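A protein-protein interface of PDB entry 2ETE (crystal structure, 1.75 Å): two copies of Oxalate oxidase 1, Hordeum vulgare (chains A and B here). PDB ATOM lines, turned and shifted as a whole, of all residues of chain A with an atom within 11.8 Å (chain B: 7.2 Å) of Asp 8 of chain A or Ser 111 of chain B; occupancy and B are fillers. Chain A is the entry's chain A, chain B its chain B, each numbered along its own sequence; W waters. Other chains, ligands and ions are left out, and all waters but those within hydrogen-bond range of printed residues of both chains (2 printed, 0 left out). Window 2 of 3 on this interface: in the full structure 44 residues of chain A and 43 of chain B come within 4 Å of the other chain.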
ATOM      1  N   PRO A   3      24.686 -10.678  -2.394  1.00  0.00           N
ATOM      2  CA  PRO A   3      26.128 -10.489  -2.210  1.00  0.00           C
ATOM      3  C   PRO A   3      26.540 -10.662  -0.739  1.00  0.00           C
ATOM      4  O   PRO A   3      25.812 -10.216   0.159  1.00  0.00           O
ATOM      5  CB  PRO A   3      26.345  -9.033  -2.646  1.00  0.00           C
ATOM      6  CG  PRO A   3      25.243  -8.758  -3.612  1.00  0.00           C
ATOM      7  CD  PRO A   3      24.059  -9.532  -3.078  1.00  0.00           C
ATOM      8  N   ASP A   4      27.686 -11.308  -0.503  1.00  0.00           N
ATOM      9  CA  ASP A   4      28.230 -11.480   0.858  1.00  0.00           C
ATOM     10  C   ASP A   4      28.590 -10.130   1.499  1.00  0.00           C
ATOM     11  O   ASP A   4      28.918  -9.173   0.785  1.00  0.00           O
ATOM     12  CB  ASP A   4      29.488 -12.367   0.836  1.00  0.00           C
ATOM     13  CG  ASP A   4      29.177 -13.868   0.812  1.00  0.00           C
ATOM     14  OD1 ASP A   4      30.119 -14.656   1.058  1.00  0.00           O
ATOM     15  OD2 ASP A   4      28.014 -14.267   0.560  1.00  0.00           O
ATOM     16  N   PRO A   5      28.546 -10.051   2.846  1.00  0.00           N
ATOM     17  CA  PRO A   5      28.966  -8.826   3.536  1.00  0.00           C
ATOM     18  C   PRO A   5      30.484  -8.630   3.486  1.00  0.00           C
ATOM     19  O   PRO A   5      31.234  -9.613   3.380  1.00  0.00           O
ATOM     20  CB  PRO A   5      28.509  -9.068   4.977  1.00  0.00           C
ATOM     21  CG  PRO A   5      28.568 -10.552   5.130  1.00  0.00           C
ATOM     22  CD  PRO A   5      28.100 -11.084   3.802  1.00  0.00           C
ATOM     23  N   LEU A   6      30.920  -7.371   3.566  1.00  0.00           N
ATOM     24  CA  LEU A   6      32.343  -7.010   3.502  1.00  0.00           C
ATOM     25  C   LEU A   6      32.863  -6.405   4.814  1.00  0.00           C
ATOM     26  O   LEU A   6      33.977  -5.870   4.869  1.00  0.00           O
ATOM     27  CB  LEU A   6      32.594  -6.062   2.317  1.00  0.00           C
ATOM     28  CG  LEU A   6      32.454  -6.716   0.933  1.00  0.00           C
ATOM     29  CD1 LEU A   6      32.320  -5.669  -0.172  1.00  0.00           C
ATOM     30  CD2 LEU A   6      33.635  -7.628   0.656  1.00  0.00           C
ATOM     31  N   GLN A   7      32.031  -6.501   5.853  1.00  0.00           N
ATOM     32  CA  GLN A   7      32.337  -6.054   7.217  1.00  0.00           C
ATOM     33  C   GLN A   7      31.295  -6.680   8.146  1.00  0.00           C
ATOM     34  O   GLN A   7      30.359  -7.343   7.670  1.00  0.00           O
ATOM     35  CB  GLN A   7      32.311  -4.518   7.330  1.00  0.00           C
ATOM     36  CG  GLN A   7      30.955  -3.862   7.008  1.00  0.00           C
ATOM     37  CD  GLN A   7      30.588  -3.953   5.533  1.00  0.00           C
ATOM     38  OE1 GLN A   7      31.342  -3.512   4.664  1.00  0.00           O
ATOM     39  NE2 GLN A   7      29.430  -4.537   5.246  1.00  0.00           N
ATOM     40  N   ASP A   8      31.446  -6.468   9.455  1.00  0.00           N
ATOM     41  CA  ASP A   8      30.545  -7.068  10.453  1.00  0.00           C
ATOM     42  C   ASP A   8      29.095  -6.600  10.315  1.00  0.00           C
ATOM     43  O   ASP A   8      28.173  -7.420  10.250  1.00  0.00           O
ATOM     44  CB  ASP A   8      31.009  -6.751  11.886  1.00  0.00           C
ATOM     45  CG  ASP A   8      32.352  -7.370  12.246  1.00  0.00           C
ATOM     46  OD1 ASP A   8      32.886  -6.965  13.303  1.00  0.00           O
ATOM     47  OD2 ASP A   8      32.878  -8.237  11.510  1.00  0.00           O
ATOM     48  N   PHE A   9      28.901  -5.278  10.295  1.00  0.00           N
ATOM     49  CA  PHE A   9      27.563  -4.668  10.341  1.00  0.00           C
ATOM     50  C   PHE A   9      27.457  -3.535   9.324  1.00  0.00           C
ATOM     51  O   PHE A   9      28.451  -2.872   9.029  1.00  0.00           O
ATOM     52  CB  PHE A   9      27.268  -4.102  11.741  1.00  0.00           C
ATOM     53  CG  PHE A   9      27.679  -5.010  12.882  1.00  0.00           C
ATOM     54  CD1 PHE A   9      28.729  -4.649  13.727  1.00  0.00           C
ATOM     55  CD2 PHE A   9      27.010  -6.211  13.117  1.00  0.00           C
ATOM     56  CE1 PHE A   9      29.116  -5.478  14.789  1.00  0.00           C
ATOM     57  CE2 PHE A   9      27.388  -7.048  14.171  1.00  0.00           C
ATOM     58  CZ  PHE A   9      28.447  -6.680  15.007  1.00  0.00           C
ATOM     59  N   CYS A  10      26.248  -3.305   8.808  1.00  0.00           N
ATOM     60  CA  CYS A  10      26.005  -2.246   7.824  1.00  0.00           C
ATOM     61  C   CYS A  10      24.504  -1.944   7.808  1.00  0.00           C
ATOM     62  O   CYS A  10      23.792  -2.340   6.885  1.00  0.00           O
ATOM     63  CB  CYS A  10      26.497  -2.690   6.434  1.00  0.00           C
ATOM     64  SG  CYS A  10      27.244  -1.398   5.376  1.00  0.00           S
ATOM     65  N   VAL A  11      24.023  -1.264   8.852  1.00  0.00           N
ATOM     66  CA  VAL A  11      22.582  -1.002   9.011  1.00  0.00           C
ATOM     67  C   VAL A  11      22.070  -0.106   7.882  1.00  0.00           C
ATOM     68  O   VAL A  11      22.639   0.958   7.628  1.00  0.00           O
ATOM     69  CB  VAL A  11      22.266  -0.350  10.388  1.00  0.00           C
ATOM     70  CG1 VAL A  11      20.760  -0.201  10.590  1.00  0.00           C
ATOM     71  CG2 VAL A  11      22.876  -1.168  11.524  1.00  0.00           C
ATOM     72  N   ALA A  12      21.014  -0.543   7.196  1.00  0.00           N
ATOM     73  CA  ALA A  12      20.451   0.237   6.087  1.00  0.00           C
ATOM     74  C   ALA A  12      20.058   1.647   6.528  1.00  0.00           C
ATOM     75  O   ALA A  12      19.380   1.822   7.545  1.00  0.00           O
ATOM     76  CB  ALA A  12      19.245  -0.476   5.480  1.00  0.00           C
ATOM     77  N   CYS A  26      24.609   2.499   4.117  1.00  0.00           N
ATOM     78  CA  CYS A  26      24.583   2.154   5.535  1.00  0.00           C
ATOM     79  C   CYS A  26      24.740   3.358   6.449  1.00  0.00           C
ATOM     80  O   CYS A  26      25.418   4.324   6.103  1.00  0.00           O
ATOM     81  CB  CYS A  26      25.687   1.143   5.849  1.00  0.00           C
ATOM     82  SG  CYS A  26      25.675  -0.275   4.743  1.00  0.00           S
ATOM     83  N   LYS A  27      24.105   3.283   7.615  1.00  0.00           N
ATOM     84  CA  LYS A  27      24.322   4.257   8.682  1.00  0.00           C
ATOM     85  C   LYS A  27      25.771   4.171   9.161  1.00  0.00           C
ATOM     86  O   LYS A  27      26.321   3.073   9.263  1.00  0.00           O
ATOM     87  CB  LYS A  27      23.392   3.961   9.867  1.00  0.00           C
ATOM     88  CG  LYS A  27      21.896   4.092   9.571  1.00  0.00           C
ATOM     89  CD  LYS A  27      21.496   5.536   9.268  1.00  0.00           C
ATOM     90  CE  LYS A  27      21.680   6.450  10.483  1.00  0.00           C
ATOM     91  NZ  LYS A  27      22.153   7.799  10.075  1.00  0.00           N
ATOM     92  N   PRO A  28      26.398   5.324   9.467  1.00  0.00           N
ATOM     93  CA  PRO A  28      27.665   5.252  10.198  1.00  0.00           C
ATOM     94  C   PRO A  28      27.448   4.461  11.490  1.00  0.00           C
ATOM     95  O   PRO A  28      26.375   4.562  12.097  1.00  0.00           O
ATOM     96  CB  PRO A  28      27.966   6.718  10.528  1.00  0.00           C
ATOM     97  CG  PRO A  28      27.222   7.505   9.520  1.00  0.00           C
ATOM     98  CD  PRO A  28      25.997   6.712   9.171  1.00  0.00           C
ATOM     99  N   MET A  29      28.437   3.668  11.899  1.00  0.00           N
ATOM    100  CA  MET A  29      28.291   2.844  13.105  1.00  0.00           C
ATOM    101  C   MET A  29      27.982   3.677  14.352  1.00  0.00           C
ATOM    102  O   MET A  29      27.261   3.222  15.240  1.00  0.00           O
ATOM    103  CB  MET A  29      29.519   1.956  13.336  1.00  0.00           C
ATOM    104  CG  MET A  29      29.656   0.777  12.363  1.00  0.00           C
ATOM    105  SD  MET A  29      28.206  -0.318  12.279  1.00  0.00           S
ATOM    106  CE  MET A  29      28.005  -0.813  13.992  1.00  0.00           C
ATOM    107  N   ALA A  32      24.207   3.855  14.629  1.00  0.00           N
ATOM    108  CA  ALA A  32      23.454   2.606  14.506  1.00  0.00           C
ATOM    109  C   ALA A  32      22.737   2.210  15.799  1.00  0.00           C
ATOM    110  O   ALA A  32      21.726   1.503  15.765  1.00  0.00           O
ATOM    111  CB  ALA A  32      24.370   1.484  14.041  1.00  0.00           C
ATOM    112  N   GLY A  33      23.256   2.666  16.936  1.00  0.00           N
ATOM    113  CA  GLY A  33      22.693   2.278  18.231  1.00  0.00           C
ATOM    114  C   GLY A  33      23.069   0.857  18.616  1.00  0.00           C
ATOM    115  O   GLY A  33      23.936   0.241  17.987  1.00  0.00           O
ATOM    116  N   PHE A  36      20.101  -2.837  16.803  1.00  0.00           N
ATOM    117  CA  PHE A  36      19.809  -3.097  15.383  1.00  0.00           C
ATOM    118  C   PHE A  36      19.733  -4.579  14.998  1.00  0.00           C
ATOM    119  O   PHE A  36      19.090  -4.929  14.004  1.00  0.00           O
ATOM    120  CB  PHE A  36      20.780  -2.339  14.462  1.00  0.00           C
ATOM    121  CG  PHE A  36      22.229  -2.672  14.681  1.00  0.00           C
ATOM    122  CD1 PHE A  36      22.834  -3.725  13.994  1.00  0.00           C
ATOM    123  CD2 PHE A  36      23.005  -1.916  15.559  1.00  0.00           C
ATOM    124  CE1 PHE A  36      24.182  -4.029  14.191  1.00  0.00           C
ATOM    125  CE2 PHE A  36      24.351  -2.212  15.762  1.00  0.00           C
ATOM    126  CZ  PHE A  36      24.943  -3.270  15.077  1.00  0.00           C
ATOM    127  N   LEU A  37      20.378  -5.440  15.784  1.00  0.00           N
ATOM    128  CA  LEU A  37      20.353  -6.886  15.536  1.00  0.00           C
ATOM    129  C   LEU A  37      19.083  -7.571  16.056  1.00  0.00           C
ATOM    130  O   LEU A  37      18.968  -8.798  15.992  1.00  0.00           O
ATOM    131  CB  LEU A  37      21.600  -7.558  16.139  1.00  0.00           C
ATOM    132  CG  LEU A  37      22.948  -7.132  15.540  1.00  0.00           C
ATOM    133  CD1 LEU A  37      24.113  -7.686  16.355  1.00  0.00           C
ATOM    134  CD2 LEU A  37      23.071  -7.544  14.061  1.00  0.00           C
ATOM    135  N   PRO A  65      16.240  -2.900   9.280  1.00  0.00           N
ATOM    136  CA  PRO A  65      17.421  -2.435   8.538  1.00  0.00           C
ATOM    137  C   PRO A  65      18.747  -3.092   8.955  1.00  0.00           C
ATOM    138  O   PRO A  65      19.701  -3.083   8.175  1.00  0.00           O
ATOM    139  CB  PRO A  65      17.443  -0.919   8.794  1.00  0.00           C
ATOM    140  CG  PRO A  65      16.566  -0.693   9.961  1.00  0.00           C
ATOM    141  CD  PRO A  65      15.567  -1.804  10.001  1.00  0.00           C
ATOM    142  N   GLY A  66      18.787  -3.679  10.150  1.00  0.00           N
ATOM    143  CA  GLY A  66      19.968  -4.416  10.626  1.00  0.00           C
ATOM    144  C   GLY A  66      20.321  -5.657   9.811  1.00  0.00           C
ATOM    145  O   GLY A  66      21.452  -6.166   9.900  1.00  0.00           O
ATOM    146  N   THR A  67      19.365  -6.156   9.024  1.00  0.00           N
ATOM    147  CA  THR A  67      19.614  -7.306   8.139  1.00  0.00           C
ATOM    148  C   THR A  67      20.393  -6.934   6.873  1.00  0.00           C
ATOM    149  O   THR A  67      20.842  -7.819   6.142  1.00  0.00           O
ATOM    150  CB  THR A  67      18.304  -8.020   7.712  1.00  0.00           C
ATOM    151  OG1 THR A  67      17.463  -7.103   6.994  1.00  0.00           O
ATOM    152  CG2 THR A  67      17.562  -8.567   8.924  1.00  0.00           C
ATOM    153  N   ASN A  68      20.540  -5.634   6.608  1.00  0.00           N
ATOM    154  CA  ASN A  68      21.255  -5.165   5.411  1.00  0.00           C
ATOM    155  C   ASN A  68      22.646  -5.795   5.287  1.00  0.00           C
ATOM    156  O   ASN A  68      23.428  -5.778   6.247  1.00  0.00           O
ATOM    157  CB  ASN A  68      21.364  -3.633   5.422  1.00  0.00           C
ATOM    158  CG  ASN A  68      21.801  -3.060   4.080  1.00  0.00           C
ATOM    159  OD1 ASN A  68      21.312  -3.469   3.020  1.00  0.00           O
ATOM    160  ND2 ASN A  68      22.701  -2.079   4.122  1.00  0.00           N
ATOM    161  N   THR A  69      22.930  -6.334   4.097  1.00  0.00           N
ATOM    162  CA  THR A  69      24.171  -7.072   3.743  1.00  0.00           C
ATOM    163  C   THR A  69      24.280  -8.499   4.299  1.00  0.00           C
ATOM    164  O   THR A  69      25.199  -9.235   3.922  1.00  0.00           O
ATOM    165  CB  THR A  69      25.503  -6.315   4.090  1.00  0.00           C
ATOM    166  OG1 THR A  69      25.788  -6.422   5.497  1.00  0.00           O
ATOM    167  CG2 THR A  69      25.442  -4.844   3.661  1.00  0.00           C
ATOM    168  N   LEU A  70      23.366  -8.888   5.190  1.00  0.00           N
ATOM    169  CA  LEU A  70      23.529 -10.155   5.928  1.00  0.00           C
ATOM    170  C   LEU A  70      22.950 -11.405   5.245  1.00  0.00           C
ATOM    171  O   LEU A  70      23.218 -12.532   5.682  1.00  0.00           O
ATOM    172  CB  LEU A  70      23.019 -10.022   7.372  1.00  0.00           C
ATOM    173  CG  LEU A  70      23.650  -8.918   8.234  1.00  0.00           C
ATOM    174  CD1 LEU A  70      23.144  -9.026   9.670  1.00  0.00           C
ATOM    175  CD2 LEU A  70      25.188  -8.954   8.205  1.00  0.00           C
ATOM    176  N   GLY A  71      22.153 -11.207   4.197  1.00  0.00           N
ATOM    177  CA  GLY A  71      21.659 -12.313   3.367  1.00  0.00           C
ATOM    178  C   GLY A  71      20.457 -13.081   3.898  1.00  0.00           C
ATOM    179  O   GLY A  71      20.210 -14.210   3.471  1.00  0.00           O
ATOM    180  N   VAL A  72      19.709 -12.465   4.815  1.00  0.00           N
ATOM    181  CA  VAL A  72      18.541 -13.089   5.453  1.00  0.00           C
ATOM    182  C   VAL A  72      17.424 -12.076   5.739  1.00  0.00           C
ATOM    183  O   VAL A  72      17.672 -10.869   5.823  1.00  0.00           O
ATOM    184  CB  VAL A  72      18.915 -13.782   6.801  1.00  0.00           C
ATOM    185  CG1 VAL A  72      19.802 -15.009   6.572  1.00  0.00           C
ATOM    186  CG2 VAL A  72      19.585 -12.790   7.760  1.00  0.00           C
ATOM    187  N   GLN A 156      17.814 -10.502   2.024  1.00  0.00           N
ATOM    188  CA  GLN A 156      17.300  -9.361   2.787  1.00  0.00           C
ATOM    189  C   GLN A 156      16.040  -8.763   2.152  1.00  0.00           C
ATOM    190  O   GLN A 156      15.310  -8.014   2.805  1.00  0.00           O
ATOM    191  CB  GLN A 156      18.369  -8.269   2.918  1.00  0.00           C
ATOM    192  CG  GLN A 156      18.680  -7.523   1.611  1.00  0.00           C
ATOM    193  CD  GLN A 156      19.766  -6.483   1.790  1.00  0.00           C
ATOM    194  OE1 GLN A 156      20.796  -6.749   2.403  1.00  0.00           O
ATOM    195  NE2 GLN A 156      19.539  -5.286   1.259  1.00  0.00           N
ATOM    196  N   LEU B 109      28.783 -10.775  19.235  1.00  0.00           N
ATOM    197  CA  LEU B 109      30.064 -10.098  19.417  1.00  0.00           C
ATOM    198  C   LEU B 109      30.679  -9.656  18.091  1.00  0.00           C
ATOM    199  O   LEU B 109      30.873 -10.471  17.186  1.00  0.00           O
ATOM    200  CB  LEU B 109      31.028 -11.012  20.183  1.00  0.00           C
ATOM    201  CG  LEU B 109      30.585 -11.309  21.622  1.00  0.00           C
ATOM    202  CD1 LEU B 109      30.620 -12.802  21.921  1.00  0.00           C
ATOM    203  CD2 LEU B 109      31.414 -10.508  22.628  1.00  0.00           C
ATOM    204  N   GLY B 110      30.981  -8.365  17.981  1.00  0.00           N
ATOM    205  CA  GLY B 110      31.717  -7.844  16.823  1.00  0.00           C
ATOM    206  C   GLY B 110      33.152  -8.354  16.801  1.00  0.00           C
ATOM    207  O   GLY B 110      33.662  -8.837  17.818  1.00  0.00           O
ATOM    208  N   SER B 111      33.802  -8.238  15.643  1.00  0.00           N
ATOM    209  CA  SER B 111      35.205  -8.638  15.479  1.00  0.00           C
ATOM    210  C   SER B 111      36.135  -7.546  16.026  1.00  0.00           C
ATOM    211  O   SER B 111      35.665  -6.564  16.607  1.00  0.00           O
ATOM    212  CB  SER B 111      35.511  -8.913  14.002  1.00  0.00           C
ATOM    213  OG  SER B 111      35.454  -7.712  13.245  1.00  0.00           O
ATOM    214  N   LEU B 112      37.444  -7.718  15.839  1.00  0.00           N
ATOM    215  CA  LEU B 112      38.425  -6.749  16.337  1.00  0.00           C
ATOM    216  C   LEU B 112      38.155  -5.328  15.840  1.00  0.00           C
ATOM    217  O   LEU B 112      38.256  -4.373  16.617  1.00  0.00           O
ATOM    218  CB  LEU B 112      39.855  -7.171  15.981  1.00  0.00           C
ATOM    219  CG  LEU B 112      40.999  -6.320  16.557  1.00  0.00           C
ATOM    220  CD1 LEU B 112      40.990  -6.352  18.087  1.00  0.00           C
ATOM    221  CD2 LEU B 112      42.350  -6.780  16.019  1.00  0.00           C
ATOM    222  N   ASP B 113      37.803  -5.205  14.559  1.00  0.00           N
ATOM    223  CA  ASP B 113      37.521  -3.904  13.928  1.00  0.00           C
ATOM    224  C   ASP B 113      36.312  -3.196  14.543  1.00  0.00           C
ATOM    225  O   ASP B 113      36.204  -1.966  14.473  1.00  0.00           O
ATOM    226  CB  ASP B 113      37.301  -4.075  12.420  1.00  0.00           C
ATOM    227  CG  ASP B 113      38.563  -3.853  11.608  1.00  0.00           C
ATOM    228  OD1 ASP B 113      39.678  -3.964  12.161  1.00  0.00           O
ATOM    229  OD2 ASP B 113      38.438  -3.573  10.390  1.00  0.00           O
ATOM    230  N   SER B 114      35.410  -3.979  15.133  1.00  0.00           N
ATOM    231  CA  SER B 114      34.236  -3.456  15.822  1.00  0.00           C
ATOM    232  C   SER B 114      34.486  -3.297  17.326  1.00  0.00           C
ATOM    233  O   SER B 114      33.542  -3.142  18.107  1.00  0.00           O
ATOM    234  CB  SER B 114      33.026  -4.367  15.565  1.00  0.00           C
ATOM    235  OG  SER B 114      32.713  -4.427  14.181  1.00  0.00           O
ATOM    236  N   GLY B 115      35.760  -3.338  17.720  1.00  0.00           N
ATOM    237  CA  GLY B 115      36.173  -3.197  19.116  1.00  0.00           C
ATOM    238  C   GLY B 115      35.709  -4.330  20.013  1.00  0.00           C
ATOM    239  O   GLY B 115      35.585  -4.150  21.228  1.00  0.00           O
ATOM    240  N   ASN B 116      35.454  -5.496  19.415  1.00  0.00           N
ATOM    241  CA  ASN B 116      34.900  -6.649  20.135  1.00  0.00           C
ATOM    242  C   ASN B 116      33.670  -6.275  20.969  1.00  0.00           C
ATOM    243  O   ASN B 116      33.518  -6.715  22.112  1.00  0.00           O
ATOM    244  CB  ASN B 116      35.980  -7.326  20.996  1.00  0.00           C
ATOM    245  CG  ASN B 116      37.107  -7.912  20.163  1.00  0.00           C
ATOM    246  OD1 ASN B 116      36.864  -8.646  19.206  1.00  0.00           O
ATOM    247  ND2 ASN B 116      38.347  -7.593  20.526  1.00  0.00           N
ATOM    248  N   LYS B 117      32.796  -5.456  20.382  1.00  0.00           N
ATOM    249  CA  LYS B 117      31.606  -4.962  21.074  1.00  0.00           C
ATOM    250  C   LYS B 117      30.580  -6.071  21.269  1.00  0.00           C
ATOM    251  O   LYS B 117      30.293  -6.828  20.339  1.00  0.00           O
ATOM    252  CB  LYS B 117      30.979  -3.791  20.301  1.00  0.00           C
ATOM    253  CG  LYS B 117      29.718  -3.204  20.949  1.00  0.00           C
ATOM    254  CD  LYS B 117      29.345  -1.842  20.362  1.00  0.00           C
ATOM    255  CE  LYS B 117      30.216  -0.720  20.929  1.00  0.00           C
ATOM    256  NZ  LYS B 117      29.894   0.606  20.310  1.00  0.00           N
ATOM    257  N   ILE B 131      22.359 -12.883  13.446  1.00  0.00           N
ATOM    258  CA  ILE B 131      23.777 -13.080  13.765  1.00  0.00           C
ATOM    259  C   ILE B 131      24.598 -13.170  12.485  1.00  0.00           C
ATOM    260  O   ILE B 131      24.523 -14.188  11.794  1.00  0.00           O
ATOM    261  CB  ILE B 131      24.021 -14.427  14.507  1.00  0.00           C
ATOM    262  CG1 ILE B 131      22.878 -14.778  15.488  1.00  0.00           C
ATOM    263  CG2 ILE B 131      25.449 -14.472  15.090  1.00  0.00           C
ATOM    264  CD1 ILE B 131      22.976 -14.197  16.856  1.00  0.00           C
ATOM    265  N   PRO B 132      25.397 -12.128  12.171  1.00  0.00           N
ATOM    266  CA  PRO B 132      26.235 -12.171  10.965  1.00  0.00           C
ATOM    267  C   PRO B 132      27.158 -13.387  10.901  1.00  0.00           C
ATOM    268  O   PRO B 132      27.686 -13.834  11.924  1.00  0.00           O
ATOM    269  CB  PRO B 132      27.071 -10.885  11.057  1.00  0.00           C
ATOM    270  CG  PRO B 132      26.255  -9.963  11.895  1.00  0.00           C
ATOM    271  CD  PRO B 132      25.552 -10.853  12.900  1.00  0.00           C
ATOM    272  N   ARG B 133      27.338 -13.896   9.685  1.00  0.00           N
ATOM    273  CA  ARG B 133      28.232 -15.009   9.386  1.00  0.00           C
ATOM    274  C   ARG B 133      29.590 -14.904  10.103  1.00  0.00           C
ATOM    275  O   ARG B 133      30.239 -13.857  10.076  1.00  0.00           O
ATOM    276  CB  ARG B 133      28.357 -15.121   7.856  1.00  0.00           C
ATOM    277  CG  ARG B 133      29.739 -15.197   7.248  1.00  0.00           C
ATOM    278  CD  ARG B 133      29.714 -14.783   5.757  1.00  0.00           C
ATOM    279  NE  ARG B 133      28.545 -15.286   5.021  1.00  0.00           N
ATOM    280  CZ  ARG B 133      28.437 -16.517   4.522  1.00  0.00           C
ATOM    281  NH1 ARG B 133      29.427 -17.389   4.679  1.00  0.00           N
ATOM    282  NH2 ARG B 133      27.333 -16.879   3.868  1.00  0.00           N
ATOM    283  N   LEU B 135      30.610 -14.657  13.246  1.00  0.00           N
ATOM    284  CA  LEU B 135      30.805 -13.934  14.515  1.00  0.00           C
ATOM    285  C   LEU B 135      30.419 -14.769  15.737  1.00  0.00           C
ATOM    286  O   LEU B 135      29.459 -15.542  15.691  1.00  0.00           O
ATOM    287  CB  LEU B 135      30.023 -12.615  14.531  1.00  0.00           C
ATOM    288  CG  LEU B 135      30.401 -11.545  13.495  1.00  0.00           C
ATOM    289  CD1 LEU B 135      29.572 -10.283  13.733  1.00  0.00           C
ATOM    290  CD2 LEU B 135      31.898 -11.225  13.504  1.00  0.00           C
ATOM    291  N   MET B 136      31.164 -14.592  16.827  1.00  0.00           N
ATOM    292  CA  MET B 136      30.881 -15.314  18.071  1.00  0.00           C
ATOM    293  C   MET B 136      29.579 -14.818  18.701  1.00  0.00           C
ATOM    294  O   MET B 136      29.299 -13.615  18.708  1.00  0.00           O
ATOM    295  CB  MET B 136      32.044 -15.168  19.060  1.00  0.00           C
ATOM    296  CG  MET B 136      32.067 -16.244  20.149  1.00  0.00           C
ATOM    297  SD  MET B 136      33.335 -15.986  21.409  1.00  0.00           S
ATOM    298  CE  MET B 136      34.847 -16.097  20.441  1.00  0.00           C
HETATM  299  O   HOH W   1      25.920 -14.120   4.657  1.00  0.00           O
HETATM  300  O   HOH W   2      35.811  -7.058  10.602  1.00  0.00           O
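Of chain B, only Gly 110 (3.8 Å), Ser 111 (2.7 Å), Ser 114 (2.7 Å), Pro 132 (3.6 Å) and Leu 135 (3.7 Å) come within 4 Å of Asp 8 of chain A. Of the printed residues of chain B, Phe 9 of chain A touches Gly 110, Ser 114, Pro 132 and Leu 135. Of the printed residues of chain B, Leu 70 of chain A touches Pro 132 (3.9 Å). Gly 110 of chain B touches just these residues of chain A: Asp 8 (3.8 Å) and Phe 9 (3.9 Å). Of chain A, only Asp 8 (2.7 Å) comes within 4 Å of Ser 111 of chain B. No residue of chain A comes within 4 Å of Leu 112 of chain B. Gly 115 of chain B touches none of the printed residues of chain A. No residue of chain A comes within 4 Å of Asn 116 of chain B. Pro 132 of chain B touches just these residues of chain A: Asp 8 (3.6 Å), Phe 9 (3.9 Å) and Leu 70 (3.9 Å). Of the printed residues of chain A, Leu 135 of chain B touches Asp 8 (3.7 Å) and Phe 9 (3.9 Å). The nearest printed residue of chain B that does not touch Asp 8 of chain A is Asp 113 of chain B (5.2 Å). The nearest printed residue of chain B that does not touch Phe 9 of chain A is Leu 109 of chain B (4.8 Å).
No position is printed for both chains. Of the 10 pairs that touch across the chains among the printed residues, none has its exchanged pair printed and touching as well.
Water W2 lies within hydrogen-bond range of OG of Ser 111 of chain B (2.7 Å) and OD2 of Asp 8 of chain A (3.3 Å). Water W1 bridges NE of Arg 133 of chain B (2.9 Å) and O of Leu 70 of chain A (3.3 Å).
OD1 of Asp 8 of chain A lies within hydrogen-bond range of OG of Ser 111 of chain B (2.7 Å). The side-chain hydroxyl (OG) of Ser 114 of chain B sits at hydrogen-bond distance from the side-chain carboxylate (OD1) of Asp 8 of chain A, at 2.7 Å.
Among the printed residues, pairs that only touch across the chains: Asp 8 of chain A with Pro 132 of chain B, Asp 8 of chain A with Leu 135 of chain B, Asp 8 of chain A with Gly 110 of chain B, Phe 9 of chain A with Ser 114 of chain B, Phe 9 of chain A with Pro 132 of chain B, Phe 9 of chain A with Gly 110 of chain B, Leu 70 of chain A with Pro 132 of chain B and Phe 9 of chain A with Leu 135 of chain B.
The backbone carbonyl oxygen of Ser 111 of chain B sits at hydrogen-bond distance from the backbone NH of Asn 116 of chain B (3.0 Å). The backbone NH of Gly 110 of chain B is in hydrogen-bond range of the backbone carbonyl oxygen of Lys 117 of chain B, at 2.9 Å. SG of Cys 10 of chain A is disulfide-bonded to SG of Cys 26 of chain A, at 2.0 Å. O of Gly 110 of chain B lies close to OD1 of Asn 116 of chain B (3.5 Å).
Of the 27 printed residues of chain A, 3 touch a printed residue of chain B. Hydrophobic or aromatic side chains of chain A that line the printed part of chain B: Phe 9 and Leu 70. Along chain A the printed residues that touch a printed residue of chain B span positions 8 to 70. Of the 14 printed residues of chain B, 5 touch a printed residue of chain A. Hydrophobic or aromatic side chains of chain B that line the printed part of chain A: Pro 132 and Leu 135. Among the printed residues, no Asp or Glu carboxylate lies within 4 Å of a Lys or Arg side-chain nitrogen of the other chain.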
